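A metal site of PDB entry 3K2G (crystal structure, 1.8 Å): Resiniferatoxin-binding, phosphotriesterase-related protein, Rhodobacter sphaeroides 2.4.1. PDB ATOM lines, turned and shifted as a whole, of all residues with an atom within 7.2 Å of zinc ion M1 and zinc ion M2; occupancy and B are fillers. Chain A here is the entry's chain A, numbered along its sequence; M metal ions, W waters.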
ATOM      1  N   HIS A  34      27.997  19.785  13.584  1.00  0.00           N
ATOM      2  CA  HIS A  34      28.255  20.900  14.488  1.00  0.00           C
ATOM      3  C   HIS A  34      29.021  20.465  15.736  1.00  0.00           C
ATOM      4  O   HIS A  34      28.430  19.992  16.706  1.00  0.00           O
ATOM      5  CB  HIS A  34      26.897  21.526  14.874  1.00  0.00           C
ATOM      6  CG  HIS A  34      26.994  22.764  15.719  1.00  0.00           C
ATOM      7  ND1 HIS A  34      26.330  23.928  15.406  1.00  0.00           N
ATOM      8  CD2 HIS A  34      27.668  23.013  16.861  1.00  0.00           C
ATOM      9  CE1 HIS A  34      26.589  24.846  16.312  1.00  0.00           C
ATOM     10  NE2 HIS A  34      27.396  24.315  17.216  1.00  0.00           N
ATOM     11  N   GLU A  35      30.344  20.630  15.686  1.00  0.00           N
ATOM     12  CA  GLU A  35      31.225  20.273  16.800  1.00  0.00           C
ATOM     13  C   GLU A  35      32.341  21.308  16.911  1.00  0.00           C
ATOM     14  O   GLU A  35      32.758  21.891  15.907  1.00  0.00           O
ATOM     15  CB  GLU A  35      31.874  18.897  16.563  1.00  0.00           C
ATOM     16  CG  GLU A  35      30.922  17.747  16.255  1.00  0.00           C
ATOM     17  CD  GLU A  35      29.959  17.456  17.387  1.00  0.00           C
ATOM     18  OE1 GLU A  35      30.265  17.815  18.546  1.00  0.00           O
ATOM     19  OE2 GLU A  35      28.905  16.851  17.125  1.00  0.00           O
ATOM     20  N   HIS A  36      32.821  21.528  18.126  1.00  0.00           N
ATOM     21  CA  HIS A  36      33.932  22.462  18.339  1.00  0.00           C
ATOM     22  C   HIS A  36      35.145  21.615  18.710  1.00  0.00           C
ATOM     23  O   HIS A  36      35.100  20.844  19.669  1.00  0.00           O
ATOM     24  CB  HIS A  36      33.582  23.447  19.439  1.00  0.00           C
ATOM     25  CG  HIS A  36      32.442  24.350  19.102  1.00  0.00           C
ATOM     26  ND1 HIS A  36      32.580  25.447  18.273  1.00  0.00           N
ATOM     27  CD2 HIS A  36      31.120  24.286  19.418  1.00  0.00           C
ATOM     28  CE1 HIS A  36      31.394  26.019  18.106  1.00  0.00           C
ATOM     29  NE2 HIS A  36      30.497  25.325  18.784  1.00  0.00           N
ATOM     30  N   ASN A  39      38.315  25.857  21.025  1.00  0.00           N
ATOM     31  CA  ASN A  39      37.556  27.072  21.214  1.00  0.00           C
ATOM     32  C   ASN A  39      37.917  27.779  22.504  1.00  0.00           C
ATOM     33  O   ASN A  39      38.733  27.296  23.297  1.00  0.00           O
ATOM     34  CB  ASN A  39      36.044  26.780  21.169  1.00  0.00           C
ATOM     35  CG  ASN A  39      35.521  26.113  22.436  1.00  0.00           C
ATOM     36  OD1 ASN A  39      36.296  25.781  23.334  1.00  0.00           O
ATOM     37  ND2 ASN A  39      34.208  25.934  22.504  1.00  0.00           N
ATOM     38  N   PRO A 106      31.899  24.911  13.407  1.00  0.00           N
ATOM     39  CA  PRO A 106      31.382  26.269  13.249  1.00  0.00           C
ATOM     40  C   PRO A 106      31.964  27.323  14.180  1.00  0.00           C
ATOM     41  O   PRO A 106      31.384  28.396  14.337  1.00  0.00           O
ATOM     42  CB  PRO A 106      29.892  26.075  13.431  1.00  0.00           C
ATOM     43  CG  PRO A 106      29.827  25.062  14.511  1.00  0.00           C
ATOM     44  CD  PRO A 106      30.956  24.089  14.201  1.00  0.00           C
ATOM     45  N   THR A 107      33.100  27.026  14.811  1.00  0.00           N
ATOM     46  CA  THR A 107      33.721  27.995  15.705  1.00  0.00           C
ATOM     47  C   THR A 107      34.098  29.200  14.842  1.00  0.00           C
ATOM     48  O   THR A 107      34.851  29.071  13.892  1.00  0.00           O
ATOM     49  CB  THR A 107      35.015  27.431  16.329  1.00  0.00           C
ATOM     50  OG1 THR A 107      34.751  26.180  16.968  1.00  0.00           O
ATOM     51  CG2 THR A 107      35.581  28.396  17.353  1.00  0.00           C
ATOM     52  N   ILE A 111      35.199  33.285  19.328  1.00  0.00           N
ATOM     53  CA  ILE A 111      35.260  32.079  20.142  1.00  0.00           C
ATOM     54  C   ILE A 111      36.440  31.137  19.853  1.00  0.00           C
ATOM     55  O   ILE A 111      36.385  29.954  20.176  1.00  0.00           O
ATOM     56  CB  ILE A 111      33.919  31.287  20.114  1.00  0.00           C
ATOM     57  CG1 ILE A 111      33.432  31.082  18.676  1.00  0.00           C
ATOM     58  CG2 ILE A 111      32.867  32.012  20.931  1.00  0.00           C
ATOM     59  CD1 ILE A 111      32.170  30.245  18.591  1.00  0.00           C
ATOM     60  N   TYR A 136      29.829  35.705  16.369  1.00  0.00           N
ATOM     61  CA  TYR A 136      28.966  34.987  17.294  1.00  0.00           C
ATOM     62  C   TYR A 136      28.109  35.953  18.129  1.00  0.00           C
ATOM     63  O   TYR A 136      27.793  37.049  17.682  1.00  0.00           O
ATOM     64  CB  TYR A 136      29.832  34.102  18.194  1.00  0.00           C
ATOM     65  CG  TYR A 136      29.095  32.964  18.842  1.00  0.00           C
ATOM     66  CD1 TYR A 136      28.209  32.179  18.109  1.00  0.00           C
ATOM     67  CD2 TYR A 136      29.320  32.631  20.168  1.00  0.00           C
ATOM     68  CE1 TYR A 136      27.566  31.080  18.691  1.00  0.00           C
ATOM     69  CE2 TYR A 136      28.693  31.546  20.759  1.00  0.00           C
ATOM     70  CZ  TYR A 136      27.815  30.775  20.022  1.00  0.00           C
ATOM     71  OH  TYR A 136      27.216  29.682  20.593  1.00  0.00           O
ATOM     72  N   LEU A 137      27.731  35.527  19.330  1.00  0.00           N
ATOM     73  CA  LEU A 137      26.902  36.354  20.216  1.00  0.00           C
ATOM     74  C   LEU A 137      27.567  37.684  20.572  1.00  0.00           C
ATOM     75  O   LEU A 137      28.787  37.776  20.650  1.00  0.00           O
ATOM     76  CB  LEU A 137      26.556  35.566  21.482  1.00  0.00           C
ATOM     77  CG  LEU A 137      25.756  34.295  21.221  1.00  0.00           C
ATOM     78  CD1 LEU A 137      25.670  33.478  22.491  1.00  0.00           C
ATOM     79  CD2 LEU A 137      24.353  34.645  20.712  1.00  0.00           C
ATOM     80  N   GLU A 177      27.462  29.655  12.510  1.00  0.00           N
ATOM     81  CA  GLU A 177      27.231  29.504  13.919  1.00  0.00           C
ATOM     82  C   GLU A 177      27.218  31.010  14.128  1.00  0.00           C
ATOM     83  O   GLU A 177      28.036  31.548  14.886  1.00  0.00           O
ATOM     84  CB  GLU A 177      28.387  28.837  14.663  1.00  0.00           C
ATOM     85  CG  GLU A 177      28.374  29.105  16.173  1.00  0.00           C
ATOM     86  CD  GLU A 177      27.727  28.052  17.086  1.00  0.00           C
ATOM     87  OE1 GLU A 177      26.495  28.081  17.302  1.00  0.00           O
ATOM     88  OE2 GLU A 177      28.486  27.214  17.637  1.00  0.00           O
ATOM     89  N   ILE A 178      26.310  31.697  13.427  1.00  0.00           N
ATOM     90  CA  ILE A 178      26.180  33.147  13.528  1.00  0.00           C
ATOM     91  C   ILE A 178      25.351  33.383  14.788  1.00  0.00           C
ATOM     92  O   ILE A 178      24.300  32.762  14.954  1.00  0.00           O
ATOM     93  CB  ILE A 178      25.456  33.757  12.290  1.00  0.00           C
ATOM     94  CG1 ILE A 178      26.257  33.472  11.018  1.00  0.00           C
ATOM     95  CG2 ILE A 178      25.270  35.276  12.461  1.00  0.00           C
ATOM     96  CD1 ILE A 178      27.670  34.018  11.064  1.00  0.00           C
ATOM     97  N   GLY A 179      25.818  34.269  15.655  1.00  0.00           N
ATOM     98  CA  GLY A 179      25.128  34.507  16.908  1.00  0.00           C
ATOM     99  C   GLY A 179      23.869  35.335  16.998  1.00  0.00           C
ATOM    100  O   GLY A 179      23.858  36.530  16.711  1.00  0.00           O
ATOM    101  N   MET A 207      24.666  28.758   8.666  1.00  0.00           N
ATOM    102  CA  MET A 207      24.302  28.112   9.917  1.00  0.00           C
ATOM    103  C   MET A 207      24.101  29.187  10.981  1.00  0.00           C
ATOM    104  O   MET A 207      24.988  30.014  11.209  1.00  0.00           O
ATOM    105  CB  MET A 207      25.417  27.159  10.350  1.00  0.00           C
ATOM    106  CG  MET A 207      25.137  26.374  11.639  1.00  0.00           C
ATOM    107  SD  MET A 207      26.582  25.203  12.051  1.00  0.00           S
ATOM    108  CE  MET A 207      26.140  23.779  10.833  1.00  0.00           C
ATOM    109  N   VAL A 208      22.944  29.181  11.620  1.00  0.00           N
ATOM    110  CA  VAL A 208      22.655  30.190  12.633  1.00  0.00           C
ATOM    111  C   VAL A 208      22.419  29.646  14.032  1.00  0.00           C
ATOM    112  O   VAL A 208      21.629  28.736  14.257  1.00  0.00           O
ATOM    113  CB  VAL A 208      21.404  31.016  12.224  1.00  0.00           C
ATOM    114  CG1 VAL A 208      21.264  32.219  13.153  1.00  0.00           C
ATOM    115  CG2 VAL A 208      21.529  31.483  10.786  1.00  0.00           C
ATOM    116  N   HIS A 209      23.131  30.228  14.993  1.00  0.00           N
ATOM    117  CA  HIS A 209      22.967  29.839  16.389  1.00  0.00           C
ATOM    118  C   HIS A 209      21.664  30.442  16.863  1.00  0.00           C
ATOM    119  O   HIS A 209      21.417  31.632  16.671  1.00  0.00           O
ATOM    120  CB  HIS A 209      24.100  30.409  17.249  1.00  0.00           C
ATOM    121  CG  HIS A 209      23.757  30.515  18.702  1.00  0.00           C
ATOM    122  ND1 HIS A 209      24.264  29.656  19.654  1.00  0.00           N
ATOM    123  CD2 HIS A 209      22.965  31.389  19.374  1.00  0.00           C
ATOM    124  CE1 HIS A 209      23.802  29.995  20.847  1.00  0.00           C
ATOM    125  NE2 HIS A 209      23.011  31.043  20.705  1.00  0.00           N
ATOM    126  N   LEU A 210      20.829  29.632  17.486  1.00  0.00           N
ATOM    127  CA  LEU A 210      19.565  30.131  17.983  1.00  0.00           C
ATOM    128  C   LEU A 210      19.511  29.971  19.486  1.00  0.00           C
ATOM    129  O   LEU A 210      20.152  29.081  20.050  1.00  0.00           O
ATOM    130  CB  LEU A 210      18.395  29.356  17.385  1.00  0.00           C
ATOM    131  CG  LEU A 210      18.078  29.492  15.901  1.00  0.00           C
ATOM    132  CD1 LEU A 210      17.025  28.454  15.519  1.00  0.00           C
ATOM    133  CD2 LEU A 210      17.568  30.881  15.616  1.00  0.00           C
ATOM    134  N   CYS A 237      20.485  26.006  14.248  1.00  0.00           N
ATOM    135  CA  CYS A 237      21.107  25.242  15.323  1.00  0.00           C
ATOM    136  C   CYS A 237      20.260  25.177  16.584  1.00  0.00           C
ATOM    137  O   CYS A 237      19.275  25.897  16.728  1.00  0.00           O
ATOM    138  CB  CYS A 237      22.456  25.843  15.715  1.00  0.00           C
ATOM    139  SG  CYS A 237      23.623  25.962  14.360  1.00  0.00           S
ATOM    140  N   HIS A 238      20.647  24.293  17.494  1.00  0.00           N
ATOM    141  CA  HIS A 238      20.002  24.137  18.791  1.00  0.00           C
ATOM    142  C   HIS A 238      18.481  23.996  18.845  1.00  0.00           C
ATOM    143  O   HIS A 238      17.812  24.695  19.604  1.00  0.00           O
ATOM    144  CB  HIS A 238      20.468  25.292  19.673  1.00  0.00           C
ATOM    145  CG  HIS A 238      21.912  25.618  19.511  1.00  0.00           C
ATOM    146  ND1 HIS A 238      22.878  24.634  19.384  1.00  0.00           N
ATOM    147  CD2 HIS A 238      22.570  26.801  19.430  1.00  0.00           C
ATOM    148  CE1 HIS A 238      24.065  25.208  19.225  1.00  0.00           C
ATOM    149  NE2 HIS A 238      23.902  26.519  19.246  1.00  0.00           N
ATOM    150  N   GLU A 260      18.601  21.484  13.131  1.00  0.00           N
ATOM    151  CA  GLU A 260      19.744  20.802  13.704  1.00  0.00           C
ATOM    152  C   GLU A 260      19.637  20.508  15.201  1.00  0.00           C
ATOM    153  O   GLU A 260      19.612  21.418  16.028  1.00  0.00           O
ATOM    154  CB  GLU A 260      21.019  21.611  13.411  1.00  0.00           C
ATOM    155  CG  GLU A 260      22.310  20.897  13.816  1.00  0.00           C
ATOM    156  CD  GLU A 260      23.550  21.690  13.435  1.00  0.00           C
ATOM    157  OE1 GLU A 260      23.933  22.605  14.199  1.00  0.00           O
ATOM    158  OE2 GLU A 260      24.132  21.425  12.368  1.00  0.00           O
ATOM    159  N   ASP A 262      21.697  19.515  17.498  1.00  0.00           N
ATOM    160  CA  ASP A 262      23.117  19.431  17.806  1.00  0.00           C
ATOM    161  C   ASP A 262      23.463  19.317  19.282  1.00  0.00           C
ATOM    162  O   ASP A 262      24.614  19.544  19.658  1.00  0.00           O
ATOM    163  CB  ASP A 262      23.828  20.664  17.211  1.00  0.00           C
ATOM    164  CG  ASP A 262      23.035  21.947  17.430  1.00  0.00           C
ATOM    165  OD1 ASP A 262      22.520  22.140  18.547  1.00  0.00           O
ATOM    166  OD2 ASP A 262      22.942  22.761  16.473  1.00  0.00           O
ATOM    167  N   MET A 263      22.498  18.967  20.120  1.00  0.00           N
ATOM    168  CA  MET A 263      22.767  18.878  21.547  1.00  0.00           C
ATOM    169  C   MET A 263      22.515  17.467  22.084  1.00  0.00           C
ATOM    170  O   MET A 263      22.197  17.277  23.256  1.00  0.00           O
ATOM    171  CB  MET A 263      21.913  19.911  22.279  1.00  0.00           C
ATOM    172  CG  MET A 263      22.050  21.310  21.672  1.00  0.00           C
ATOM    173  SD  MET A 263      20.747  22.615  22.347  1.00  0.00           S
ATOM    174  CE  MET A 263      22.030  24.036  22.852  1.00  0.00           C
ATOM    175  N   ASP A 304      27.554  19.273  19.635  1.00  0.00           N
ATOM    176  CA  ASP A 304      27.933  20.644  19.997  1.00  0.00           C
ATOM    177  C   ASP A 304      28.930  20.576  21.144  1.00  0.00           C
ATOM    178  O   ASP A 304      28.829  21.302  22.128  1.00  0.00           O
ATOM    179  CB  ASP A 304      26.746  21.541  20.387  1.00  0.00           C
ATOM    180  CG  ASP A 304      27.133  23.026  20.467  1.00  0.00           C
ATOM    181  OD1 ASP A 304      28.118  23.403  19.806  1.00  0.00           O
ATOM    182  OD2 ASP A 304      26.466  23.819  21.175  1.00  0.00           O
ATOM    183  N   VAL A 305      29.905  19.678  21.029  1.00  0.00           N
ATOM    184  CA  VAL A 305      30.929  19.592  22.055  1.00  0.00           C
ATOM    185  C   VAL A 305      31.535  20.992  22.101  1.00  0.00           C
ATOM    186  O   VAL A 305      31.997  21.497  21.076  1.00  0.00           O
ATOM    187  CB  VAL A 305      32.030  18.602  21.668  1.00  0.00           C
ATOM    188  CG1 VAL A 305      33.200  18.702  22.629  1.00  0.00           C
ATOM    189  CG2 VAL A 305      31.459  17.174  21.673  1.00  0.00           C
ATOM    190  N   PHE A 306      31.518  21.627  23.282  1.00  0.00           N
ATOM    191  CA  PHE A 306      32.105  22.962  23.376  1.00  0.00           C
ATOM    192  C   PHE A 306      32.797  23.276  24.709  1.00  0.00           C
ATOM    193  O   PHE A 306      33.290  24.385  24.906  1.00  0.00           O
ATOM    194  CB  PHE A 306      31.053  24.034  23.043  1.00  0.00           C
ATOM    195  CG  PHE A 306      30.147  24.385  24.180  1.00  0.00           C
ATOM    196  CD1 PHE A 306      30.403  25.489  24.982  1.00  0.00           C
ATOM    197  CD2 PHE A 306      29.019  23.608  24.447  1.00  0.00           C
ATOM    198  CE1 PHE A 306      29.545  25.829  26.025  1.00  0.00           C
ATOM    199  CE2 PHE A 306      28.155  23.937  25.485  1.00  0.00           C
ATOM    200  CZ  PHE A 306      28.422  25.047  26.280  1.00  0.00           C
HETATM  201 ZN    ZN M   1      28.330  25.424  18.798  1.00  0.00          ZN
HETATM  202 ZN    ZN M   2      25.818  27.894  19.450  1.00  0.00          ZN
HETATM  203  O   HOH W   1      25.803  27.785  21.826  1.00  0.00           O
HETATM  204  O   HOH W   2      29.027  26.764  21.649  1.00  0.00           O
HETATM  205  O   HOH W   3      27.068  26.305  20.221  1.00  0.00           O
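Zinc ion M1 is bound by water W3 (2.1 Å), OE2 of Glu 177 (2.1 Å), NE2 of His 34 (2.1 Å), NE2 of His 36 (2.2 Å) and OD1 of Asp 304 (2.3 Å).
Zinc ion M1 has five donor atoms within binding distance.
The backbone NH (N) of Asp 304 is in hydrogen-bond range of the backbone carbonyl oxygen (O) of Asp 262 (3.0 Å).
The backbone NH of His 36 lies close to the backbone carbonyl oxygen of Val 305 (3.1 Å).
The backbone NH (N) of His 209 is in hydrogen-bond range of the backbone carbonyl oxygen (O) of Ile 178 (2.8 Å).
The side-chain carboxylate of Asp 262 lies within hydrogen-bond range of a ring nitrogen (ND1) of His 238, at 2.7 Å.
The backbone carbonyl oxygen (O) of Met 207 lies within hydrogen-bond range of the backbone NH (N) of Glu 177 (2.8 Å).
A ring nitrogen (ND1) of His 34 sits at hydrogen-bond distance from the side-chain sulfur (SG) of Cys 237 (3.5 Å).
The backbone carbonyl oxygen (O) of Glu 260 sits at hydrogen-bond distance from the backbone NH (N) of His 238.
ND1 of His 34 is in hydrogen-bond range of OE1 of Glu 260 (3.0 Å).
Zinc ion M2 is bound by water W3 (2.2 Å), OE1 of Glu 177 (2.3 Å), ND1 of His 209 (2.4 Å), NE2 of His 238 (2.4 Å), water W1 (2.4 Å) and OH of Tyr 136 (2.5 Å).
Zinc ion M2 has six donor atoms within binding distance.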
